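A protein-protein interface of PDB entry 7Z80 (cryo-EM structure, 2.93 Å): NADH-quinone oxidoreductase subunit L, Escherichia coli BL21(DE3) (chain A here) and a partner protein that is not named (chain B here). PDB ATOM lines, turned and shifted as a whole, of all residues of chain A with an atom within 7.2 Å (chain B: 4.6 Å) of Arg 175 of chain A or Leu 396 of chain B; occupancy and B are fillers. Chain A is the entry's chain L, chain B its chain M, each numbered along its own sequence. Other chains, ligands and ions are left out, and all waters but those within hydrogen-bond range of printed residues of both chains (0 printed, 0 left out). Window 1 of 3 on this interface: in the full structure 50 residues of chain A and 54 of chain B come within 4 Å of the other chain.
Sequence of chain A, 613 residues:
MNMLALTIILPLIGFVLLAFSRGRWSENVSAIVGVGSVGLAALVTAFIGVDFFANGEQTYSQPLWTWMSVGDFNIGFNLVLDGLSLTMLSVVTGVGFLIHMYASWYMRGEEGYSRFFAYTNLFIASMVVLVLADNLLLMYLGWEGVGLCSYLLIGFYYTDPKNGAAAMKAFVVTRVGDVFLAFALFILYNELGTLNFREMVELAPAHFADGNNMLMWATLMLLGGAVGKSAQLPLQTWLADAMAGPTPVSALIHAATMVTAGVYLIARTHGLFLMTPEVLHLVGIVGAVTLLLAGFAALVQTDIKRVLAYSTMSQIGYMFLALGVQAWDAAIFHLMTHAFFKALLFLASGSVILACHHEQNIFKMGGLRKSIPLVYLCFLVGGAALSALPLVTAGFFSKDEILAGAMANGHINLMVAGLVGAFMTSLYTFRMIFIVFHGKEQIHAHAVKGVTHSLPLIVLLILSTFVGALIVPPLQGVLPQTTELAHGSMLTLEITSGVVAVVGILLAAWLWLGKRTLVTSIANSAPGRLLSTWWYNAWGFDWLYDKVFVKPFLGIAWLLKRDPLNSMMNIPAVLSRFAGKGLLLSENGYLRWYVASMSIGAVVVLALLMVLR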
ATOM      1  N   TYR A 140     -17.655  14.473 -22.729  1.00  0.00           N
ATOM      2  CA  TYR A 140     -16.286  14.862 -23.047  1.00  0.00           C
ATOM      3  C   TYR A 140     -16.154  15.293 -24.503  1.00  0.00           C
ATOM      4  O   TYR A 140     -15.353  16.176 -24.822  1.00  0.00           O
ATOM      5  CB  TYR A 140     -15.333  13.709 -22.739  1.00  0.00           C
ATOM      6  CG  TYR A 140     -13.898  14.135 -22.552  1.00  0.00           C
ATOM      7  CD1 TYR A 140     -13.043  14.262 -23.636  1.00  0.00           C
ATOM      8  CD2 TYR A 140     -13.399  14.410 -21.288  1.00  0.00           C
ATOM      9  CE1 TYR A 140     -11.732  14.651 -23.468  1.00  0.00           C
ATOM     10  CE2 TYR A 140     -12.090  14.799 -21.110  1.00  0.00           C
ATOM     11  CZ  TYR A 140     -11.260  14.917 -22.203  1.00  0.00           C
ATOM     12  OH  TYR A 140      -9.953  15.305 -22.031  1.00  0.00           O
ATOM     13  N   GLU A 144     -14.763  18.916 -25.507  1.00  0.00           N
ATOM     14  CA  GLU A 144     -13.694  19.164 -26.468  1.00  0.00           C
ATOM     15  C   GLU A 144     -14.165  20.024 -27.632  1.00  0.00           C
ATOM     16  O   GLU A 144     -13.413  20.875 -28.117  1.00  0.00           O
ATOM     17  CB  GLU A 144     -13.148  17.833 -26.975  1.00  0.00           C
ATOM     18  CG  GLU A 144     -12.208  17.058 -26.037  1.00  0.00           C
ATOM     19  CD  GLU A 144     -10.901  17.768 -25.703  1.00  0.00           C
ATOM     20  OE1 GLU A 144     -10.901  18.824 -25.046  1.00  0.00           O
ATOM     21  OE2 GLU A 144      -9.842  17.247 -26.111  1.00  0.00           O
ATOM     22  N   LEU A 148     -12.572  23.580 -28.640  1.00  0.00           N
ATOM     23  CA  LEU A 148     -12.048  23.849 -29.977  1.00  0.00           C
ATOM     24  C   LEU A 148     -12.728  25.058 -30.605  1.00  0.00           C
ATOM     25  O   LEU A 148     -12.070  25.882 -31.250  1.00  0.00           O
ATOM     26  CB  LEU A 148     -12.214  22.625 -30.877  1.00  0.00           C
ATOM     27  CG  LEU A 148     -11.829  22.866 -32.343  1.00  0.00           C
ATOM     28  CD1 LEU A 148     -10.347  23.196 -32.448  1.00  0.00           C
ATOM     29  CD2 LEU A 148     -12.192  21.708 -33.256  1.00  0.00           C
ATOM     30  N   TYR A 151     -11.270  28.111 -29.082  1.00  0.00           N
ATOM     31  CA  TYR A 151      -9.982  28.416 -29.702  1.00  0.00           C
ATOM     32  C   TYR A 151     -10.150  29.039 -31.083  1.00  0.00           C
ATOM     33  O   TYR A 151      -9.461  30.008 -31.423  1.00  0.00           O
ATOM     34  CB  TYR A 151      -9.137  27.146 -29.795  1.00  0.00           C
ATOM     35  CG  TYR A 151      -8.090  27.172 -30.888  1.00  0.00           C
ATOM     36  CD1 TYR A 151      -6.933  27.928 -30.758  1.00  0.00           C
ATOM     37  CD2 TYR A 151      -8.264  26.434 -32.054  1.00  0.00           C
ATOM     38  CE1 TYR A 151      -5.981  27.953 -31.759  1.00  0.00           C
ATOM     39  CE2 TYR A 151      -7.321  26.455 -33.059  1.00  0.00           C
ATOM     40  CZ  TYR A 151      -6.183  27.214 -32.907  1.00  0.00           C
ATOM     41  OH  TYR A 151      -5.244  27.226 -33.911  1.00  0.00           O
ATOM     42  N   LYS A 169      -3.128  29.997 -25.751  1.00  0.00           N
ATOM     43  CA  LYS A 169      -3.059  29.871 -24.297  1.00  0.00           C
ATOM     44  C   LYS A 169      -4.366  29.335 -23.725  1.00  0.00           C
ATOM     45  O   LYS A 169      -4.354  28.475 -22.829  1.00  0.00           O
ATOM     46  CB  LYS A 169      -2.718  31.221 -23.669  1.00  0.00           C
ATOM     47  CG  LYS A 169      -2.668  31.208 -22.151  1.00  0.00           C
ATOM     48  CD  LYS A 169      -2.921  32.591 -21.581  1.00  0.00           C
ATOM     49  CE  LYS A 169      -1.634  33.383 -21.462  1.00  0.00           C
ATOM     50  NZ  LYS A 169      -1.867  34.844 -21.633  1.00  0.00           N
ATOM     51  N   ALA A 170      -5.500  29.823 -24.242  1.00  0.00           N
ATOM     52  CA  ALA A 170      -6.800  29.335 -23.793  1.00  0.00           C
ATOM     53  C   ALA A 170      -6.976  27.857 -24.107  1.00  0.00           C
ATOM     54  O   ALA A 170      -7.447  27.087 -23.258  1.00  0.00           O
ATOM     55  CB  ALA A 170      -7.917  30.156 -24.434  1.00  0.00           C
ATOM     56  N   PHE A 171      -6.578  27.435 -25.312  1.00  0.00           N
ATOM     57  CA  PHE A 171      -6.696  26.024 -25.664  1.00  0.00           C
ATOM     58  C   PHE A 171      -5.770  25.161 -24.817  1.00  0.00           C
ATOM     59  O   PHE A 171      -6.138  24.044 -24.445  1.00  0.00           O
ATOM     60  CB  PHE A 171      -6.423  25.813 -27.149  1.00  0.00           C
ATOM     61  CG  PHE A 171      -6.933  24.498 -27.675  1.00  0.00           C
ATOM     62  CD1 PHE A 171      -8.288  24.297 -27.876  1.00  0.00           C
ATOM     63  CD2 PHE A 171      -6.060  23.464 -27.963  1.00  0.00           C
ATOM     64  CE1 PHE A 171      -8.761  23.092 -28.358  1.00  0.00           C
ATOM     65  CE2 PHE A 171      -6.528  22.257 -28.447  1.00  0.00           C
ATOM     66  CZ  PHE A 171      -7.880  22.072 -28.643  1.00  0.00           C
ATOM     67  N   VAL A 172      -4.587  25.672 -24.466  1.00  0.00           N
ATOM     68  CA  VAL A 172      -3.651  24.895 -23.656  1.00  0.00           C
ATOM     69  C   VAL A 172      -4.195  24.685 -22.244  1.00  0.00           C
ATOM     70  O   VAL A 172      -4.190  23.559 -21.726  1.00  0.00           O
ATOM     71  CB  VAL A 172      -2.265  25.568 -23.643  1.00  0.00           C
ATOM     72  CG1 VAL A 172      -1.430  25.081 -22.466  1.00  0.00           C
ATOM     73  CG2 VAL A 172      -1.534  25.284 -24.942  1.00  0.00           C
ATOM     74  N   VAL A 173      -4.691  25.752 -21.606  1.00  0.00           N
ATOM     75  CA  VAL A 173      -5.184  25.592 -20.235  1.00  0.00           C
ATOM     76  C   VAL A 173      -6.467  24.765 -20.212  1.00  0.00           C
ATOM     77  O   VAL A 173      -6.682  23.958 -19.294  1.00  0.00           O
ATOM     78  CB  VAL A 173      -5.372  26.951 -19.530  1.00  0.00           C
ATOM     79  CG1 VAL A 173      -4.033  27.599 -19.256  1.00  0.00           C
ATOM     80  CG2 VAL A 173      -6.250  27.863 -20.325  1.00  0.00           C
ATOM     81  N   THR A 174      -7.330  24.922 -21.226  1.00  0.00           N
ATOM     82  CA  THR A 174      -8.522  24.087 -21.270  1.00  0.00           C
ATOM     83  C   THR A 174      -8.174  22.632 -21.546  1.00  0.00           C
ATOM     84  O   THR A 174      -8.820  21.745 -20.994  1.00  0.00           O
ATOM     85  CB  THR A 174      -9.514  24.606 -22.307  1.00  0.00           C
ATOM     86  OG1 THR A 174      -8.837  24.856 -23.542  1.00  0.00           O
ATOM     87  CG2 THR A 174     -10.165  25.888 -21.818  1.00  0.00           C
ATOM     88  N   ARG A 175      -7.146  22.361 -22.357  1.00  0.00           N
ATOM     89  CA  ARG A 175      -6.729  20.980 -22.576  1.00  0.00           C
ATOM     90  C   ARG A 175      -6.122  20.369 -21.320  1.00  0.00           C
ATOM     91  O   ARG A 175      -6.283  19.168 -21.083  1.00  0.00           O
ATOM     92  CB  ARG A 175      -5.739  20.899 -23.737  1.00  0.00           C
ATOM     93  CG  ARG A 175      -6.391  20.872 -25.109  1.00  0.00           C
ATOM     94  CD  ARG A 175      -7.011  19.519 -25.417  1.00  0.00           C
ATOM     95  NE  ARG A 175      -6.004  18.538 -25.805  1.00  0.00           N
ATOM     96  CZ  ARG A 175      -6.275  17.307 -26.216  1.00  0.00           C
ATOM     97  NH1 ARG A 175      -7.518  16.865 -26.305  1.00  0.00           N
ATOM     98  NH2 ARG A 175      -5.272  16.498 -26.546  1.00  0.00           N
ATOM     99  N   VAL A 176      -5.438  21.172 -20.505  1.00  0.00           N
ATOM    100  CA  VAL A 176      -4.931  20.678 -19.225  1.00  0.00           C
ATOM    101  C   VAL A 176      -6.088  20.315 -18.295  1.00  0.00           C
ATOM    102  O   VAL A 176      -6.104  19.241 -17.667  1.00  0.00           O
ATOM    103  CB  VAL A 176      -3.994  21.721 -18.589  1.00  0.00           C
ATOM    104  CG1 VAL A 176      -3.731  21.386 -17.151  1.00  0.00           C
ATOM    105  CG2 VAL A 176      -2.686  21.792 -19.356  1.00  0.00           C
ATOM    106  N   GLY A 177      -7.090  21.197 -18.216  1.00  0.00           N
ATOM    107  CA  GLY A 177      -8.278  20.884 -17.434  1.00  0.00           C
ATOM    108  C   GLY A 177      -9.021  19.666 -17.952  1.00  0.00           C
ATOM    109  O   GLY A 177      -9.531  18.855 -17.175  1.00  0.00           O
ATOM    110  N   ASP A 178      -9.066  19.501 -19.272  1.00  0.00           N
ATOM    111  CA  ASP A 178      -9.749  18.350 -19.845  1.00  0.00           C
ATOM    112  C   ASP A 178      -8.945  17.072 -19.665  1.00  0.00           C
ATOM    113  O   ASP A 178      -9.517  15.982 -19.648  1.00  0.00           O
ATOM    114  CB  ASP A 178     -10.052  18.612 -21.316  1.00  0.00           C
ATOM    115  CG  ASP A 178     -10.993  19.777 -21.497  1.00  0.00           C
ATOM    116  OD1 ASP A 178     -11.301  20.437 -20.482  1.00  0.00           O
ATOM    117  OD2 ASP A 178     -11.430  20.047 -22.629  1.00  0.00           O
ATOM    118  N   VAL A 179      -7.627  17.179 -19.514  1.00  0.00           N
ATOM    119  CA  VAL A 179      -6.831  16.015 -19.138  1.00  0.00           C
ATOM    120  C   VAL A 179      -7.125  15.614 -17.695  1.00  0.00           C
ATOM    121  O   VAL A 179      -7.200  14.420 -17.368  1.00  0.00           O
ATOM    122  CB  VAL A 179      -5.341  16.304 -19.399  1.00  0.00           C
ATOM    123  CG1 VAL A 179      -4.435  15.501 -18.492  1.00  0.00           C
ATOM    124  CG2 VAL A 179      -5.027  15.994 -20.849  1.00  0.00           C
ATOM    125  N   PHE A 180      -7.339  16.601 -16.818  1.00  0.00           N
ATOM    126  CA  PHE A 180      -7.813  16.283 -15.467  1.00  0.00           C
ATOM    127  C   PHE A 180      -9.192  15.615 -15.501  1.00  0.00           C
ATOM    128  O   PHE A 180      -9.459  14.658 -14.756  1.00  0.00           O
ATOM    129  CB  PHE A 180      -7.865  17.547 -14.608  1.00  0.00           C
ATOM    130  CG  PHE A 180      -6.530  18.211 -14.401  1.00  0.00           C
ATOM    131  CD1 PHE A 180      -5.376  17.464 -14.217  1.00  0.00           C
ATOM    132  CD2 PHE A 180      -6.440  19.590 -14.340  1.00  0.00           C
ATOM    133  CE1 PHE A 180      -4.157  18.081 -14.008  1.00  0.00           C
ATOM    134  CE2 PHE A 180      -5.228  20.211 -14.127  1.00  0.00           C
ATOM    135  CZ  PHE A 180      -4.084  19.454 -13.964  1.00  0.00           C
ATOM    136  N   LEU A 181     -10.075  16.108 -16.374  1.00  0.00           N
ATOM    137  CA  LEU A 181     -11.385  15.489 -16.566  1.00  0.00           C
ATOM    138  C   LEU A 181     -11.256  14.064 -17.096  1.00  0.00           C
ATOM    139  O   LEU A 181     -12.030  13.175 -16.715  1.00  0.00           O
ATOM    140  CB  LEU A 181     -12.218  16.342 -17.520  1.00  0.00           C
ATOM    141  CG  LEU A 181     -13.659  15.919 -17.793  1.00  0.00           C
ATOM    142  CD1 LEU A 181     -14.460  15.857 -16.511  1.00  0.00           C
ATOM    143  CD2 LEU A 181     -14.292  16.878 -18.773  1.00  0.00           C
ATOM    144  N   GLY A 228     -10.815  24.093 -14.807  1.00  0.00           N
ATOM    145  CA  GLY A 228     -10.176  24.349 -16.085  1.00  0.00           C
ATOM    146  C   GLY A 228     -11.121  24.970 -17.095  1.00  0.00           C
ATOM    147  O   GLY A 228     -10.764  25.929 -17.783  1.00  0.00           O
ATOM    148  N   LYS A 229     -12.341  24.440 -17.192  1.00  0.00           N
ATOM    149  CA  LYS A 229     -13.279  24.954 -18.185  1.00  0.00           C
ATOM    150  C   LYS A 229     -13.920  26.274 -17.769  1.00  0.00           C
ATOM    151  O   LYS A 229     -14.176  27.128 -18.626  1.00  0.00           O
ATOM    152  CB  LYS A 229     -14.358  23.910 -18.468  1.00  0.00           C
ATOM    153  CG  LYS A 229     -15.230  24.218 -19.667  1.00  0.00           C
ATOM    154  CD  LYS A 229     -14.408  24.396 -20.928  1.00  0.00           C
ATOM    155  CE  LYS A 229     -13.827  23.089 -21.425  1.00  0.00           C
ATOM    156  NZ  LYS A 229     -13.061  23.262 -22.690  1.00  0.00           N
ATOM    157  N   LEU A 235      -6.764  27.671 -12.900  1.00  0.00           N
ATOM    158  CA  LEU A 235      -6.679  27.728 -14.356  1.00  0.00           C
ATOM    159  C   LEU A 235      -7.534  28.856 -14.923  1.00  0.00           C
ATOM    160  O   LEU A 235      -8.235  28.690 -15.922  1.00  0.00           O
ATOM    161  CB  LEU A 235      -7.072  26.388 -14.972  1.00  0.00           C
ATOM    162  CG  LEU A 235      -6.082  25.251 -14.713  1.00  0.00           C
ATOM    163  CD1 LEU A 235      -6.665  23.909 -15.107  1.00  0.00           C
ATOM    164  CD2 LEU A 235      -4.777  25.504 -15.452  1.00  0.00           C
ATOM    165  N   ALA B 392      -4.753  18.983 -38.475  1.00  0.00           N
ATOM    166  CA  ALA B 392      -4.019  19.315 -37.261  1.00  0.00           C
ATOM    167  C   ALA B 392      -4.903  19.195 -36.027  1.00  0.00           C
ATOM    168  O   ALA B 392      -4.410  18.881 -34.939  1.00  0.00           O
ATOM    169  CB  ALA B 392      -3.433  20.721 -37.369  1.00  0.00           C
ATOM    170  N   VAL B 393      -6.204  19.451 -36.178  1.00  0.00           N
ATOM    171  CA  VAL B 393      -7.153  19.194 -35.102  1.00  0.00           C
ATOM    172  C   VAL B 393      -7.287  17.693 -34.862  1.00  0.00           C
ATOM    173  O   VAL B 393      -7.360  17.234 -33.717  1.00  0.00           O
ATOM    174  CB  VAL B 393      -8.502  19.860 -35.443  1.00  0.00           C
ATOM    175  CG1 VAL B 393      -9.677  19.139 -34.803  1.00  0.00           C
ATOM    176  CG2 VAL B 393      -8.481  21.321 -35.032  1.00  0.00           C
ATOM    177  N   ALA B 394      -7.293  16.906 -35.938  1.00  0.00           N
ATOM    178  CA  ALA B 394      -7.399  15.457 -35.812  1.00  0.00           C
ATOM    179  C   ALA B 394      -6.176  14.858 -35.126  1.00  0.00           C
ATOM    180  O   ALA B 394      -6.305  13.933 -34.316  1.00  0.00           O
ATOM    181  CB  ALA B 394      -7.602  14.826 -37.189  1.00  0.00           C
ATOM    182  N   THR B 395      -4.982  15.372 -35.425  1.00  0.00           N
ATOM    183  CA  THR B 395      -3.765  14.769 -34.892  1.00  0.00           C
ATOM    184  C   THR B 395      -3.518  15.080 -33.420  1.00  0.00           C
ATOM    185  O   THR B 395      -2.644  14.448 -32.818  1.00  0.00           O
ATOM    186  CB  THR B 395      -2.545  15.208 -35.704  1.00  0.00           C
ATOM    187  OG1 THR B 395      -2.700  16.571 -36.110  1.00  0.00           O
ATOM    188  CG2 THR B 395      -2.383  14.331 -36.935  1.00  0.00           C
ATOM    189  N   LEU B 396      -4.241  16.025 -32.821  1.00  0.00           N
ATOM    190  CA  LEU B 396      -4.066  16.297 -31.400  1.00  0.00           C
ATOM    191  C   LEU B 396      -5.006  15.481 -30.523  1.00  0.00           C
ATOM    192  O   LEU B 396      -5.000  15.658 -29.301  1.00  0.00           O
ATOM    193  CB  LEU B 396      -4.234  17.800 -31.105  1.00  0.00           C
ATOM    194  CG  LEU B 396      -5.417  18.664 -31.564  1.00  0.00           C
ATOM    195  CD1 LEU B 396      -6.677  18.459 -30.726  1.00  0.00           C
ATOM    196  CD2 LEU B 396      -5.037  20.135 -31.577  1.00  0.00           C
ATOM    197  N   GLY B 397      -5.811  14.601 -31.112  1.00  0.00           N
ATOM    198  CA  GLY B 397      -6.705  13.762 -30.340  1.00  0.00           C
ATOM    199  C   GLY B 397      -8.071  14.377 -30.137  1.00  0.00           C
ATOM    200  O   GLY B 397      -8.559  14.460 -29.006  1.00  0.00           O
ATOM    201  N   MET B 398      -8.697  14.811 -31.219  1.00  0.00           N
ATOM    202  CA  MET B 398      -9.968  15.509 -31.076  1.00  0.00           C
ATOM    203  C   MET B 398     -11.134  14.559 -31.327  1.00  0.00           C
ATOM    204  O   MET B 398     -11.096  13.787 -32.294  1.00  0.00           O
ATOM    205  CB  MET B 398     -10.047  16.687 -32.031  1.00  0.00           C
ATOM    206  CG  MET B 398     -11.397  17.346 -32.044  1.00  0.00           C
ATOM    207  SD  MET B 398     -11.429  18.834 -31.047  1.00  0.00           S
ATOM    208  CE  MET B 398     -13.193  19.052 -30.935  1.00  0.00           C
ATOM    209  N   LEU B 429      -0.544  14.067 -24.338  1.00  0.00           N
ATOM    210  CA  LEU B 429      -1.592  14.572 -25.229  1.00  0.00           C
ATOM    211  C   LEU B 429      -1.718  16.090 -25.143  1.00  0.00           C
ATOM    212  O   LEU B 429      -2.006  16.754 -26.150  1.00  0.00           O
ATOM    213  CB  LEU B 429      -2.938  13.920 -24.916  1.00  0.00           C
ATOM    214  CG  LEU B 429      -3.217  12.560 -25.545  1.00  0.00           C
ATOM    215  CD1 LEU B 429      -4.383  11.885 -24.850  1.00  0.00           C
ATOM    216  CD2 LEU B 429      -3.487  12.716 -27.032  1.00  0.00           C
ATOM    217  N   VAL B 430      -1.537  16.650 -23.943  1.00  0.00           N
ATOM    218  CA  VAL B 430      -1.483  18.112 -23.811  1.00  0.00           C
ATOM    219  C   VAL B 430      -0.334  18.680 -24.646  1.00  0.00           C
ATOM    220  O   VAL B 430      -0.495  19.668 -25.379  1.00  0.00           O
ATOM    221  CB  VAL B 430      -1.374  18.525 -22.331  1.00  0.00           C
ATOM    222  CG1 VAL B 430      -0.653  19.859 -22.173  1.00  0.00           C
ATOM    223  CG2 VAL B 430      -2.743  18.644 -21.726  1.00  0.00           C
ATOM    224  N   ALA B 432       0.898  17.278 -27.258  1.00  0.00           N
ATOM    225  CA  ALA B 432       0.504  17.093 -28.652  1.00  0.00           C
ATOM    226  C   ALA B 432      -0.365  18.242 -29.142  1.00  0.00           C
ATOM    227  O   ALA B 432      -0.174  18.751 -30.257  1.00  0.00           O
ATOM    228  CB  ALA B 432      -0.227  15.762 -28.821  1.00  0.00           C
ATOM    229  N   SER B 433      -1.321  18.664 -28.312  1.00  0.00           N
ATOM    230  CA  SER B 433      -2.119  19.844 -28.629  1.00  0.00           C
ATOM    231  C   SER B 433      -1.239  21.081 -28.768  1.00  0.00           C
ATOM    232  O   SER B 433      -1.468  21.917 -29.651  1.00  0.00           O
ATOM    233  CB  SER B 433      -3.181  20.064 -27.554  1.00  0.00           C
ATOM    234  OG  SER B 433      -3.559  21.427 -27.496  1.00  0.00           O
ATOM    235  N   SER B 436       0.543  20.944 -32.136  1.00  0.00           N
ATOM    236  CA  SER B 436      -0.399  21.146 -33.236  1.00  0.00           C
ATOM    237  C   SER B 436      -0.785  22.614 -33.373  1.00  0.00           C
ATOM    238  O   SER B 436      -0.829  23.151 -34.490  1.00  0.00           O
ATOM    239  CB  SER B 436      -1.639  20.278 -33.030  1.00  0.00           C
ATOM    240  OG  SER B 436      -1.330  18.907 -33.200  1.00  0.00           O
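The backbone carbonyl oxygen (O) of Phe 171 of chain A lies within hydrogen-bond range of the side-chain hydroxyl (OG1) of Thr 174 of chain A (3.0 Å).
Printed residues of chain B that touch a printed residue of chain A: Val 393, Leu 396, Gly 397, Met 398, Leu 429, Val 430 and Ser 433.
Along chain B the printed residues that touch a printed residue of chain A span positions 393 to 433.
Printed residues of chain A that touch a printed residue of chain B: Glu 144, Leu 148, Phe 171, Arg 175, Val 176 and Val 179.
Hydrophobic or aromatic side chains of chain A that line the printed part of chain B: Leu 148, Phe 171, Val 176 and Val 179.
NH2 of Arg 175 of chain A sits at hydrogen-bond distance from O of Leu 429 of chain B, at 3.3 Å.
O of Leu 396 of chain B lies within hydrogen-bond range of NH2 of Arg 175 of chain A (2.9 Å).
Met 398 of chain B touches Glu 144 of chain A (CE to O, 3.4 Å).
Leu 148 of chain A touches Val 393 of chain B (CD1 to CG2, 3.7 Å).
CD2 of Leu 148 of chain A touches CE of Met 398 of chain B, at 3.7 Å.
CE2 of Phe 171 of chain A touches OG of Ser 433 of chain B (3.2 Å).
Gly 397 of chain B touches Arg 175 of chain A.
O of Arg 175 of chain A touches CG2 of Val 430 of chain B (3.6 Å).
NE of Arg 175 of chain A touches CB of Ser 433 of chain B (3.7 Å).
Val 430 of chain B touches Val 176 of chain A (CG2 to N, 3.9 Å).
CG2 of Val 179 of chain A touches CG2 of Val 430 of chain B, 3.6 Å away.
Arg 175 of chain A touches just these residues of chain B: Leu 396, Gly 397, Leu 429, Val 430 and Ser 433.
Of the printed residues of chain A, Met 398 of chain B touches Glu 144 (3.4 Å) and Leu 148 (3.7 Å).
Printed residues of chain B within 4 Å of Leu 148 of chain A: Val 393 and Met 398.
Of the printed residues of chain B, Phe 171 of chain A touches Ser 433.
Printed residues of chain B within 4 Å of Val 176 of chain A: Val 430.
Ala 170 of chain A touches none of the printed residues of chain B.
The nearest printed residue of chain B that does not touch Arg 175 of chain A is Met 398 of chain B (5.5 Å).
The nearest residue of chain A that does not touch Leu 396 of chain B is Phe 171 of chain A (4.1 Å).
The nearest printed residue of chain A that does not touch Val 430 of chain B is Val 172 of chain A (5.1 Å).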
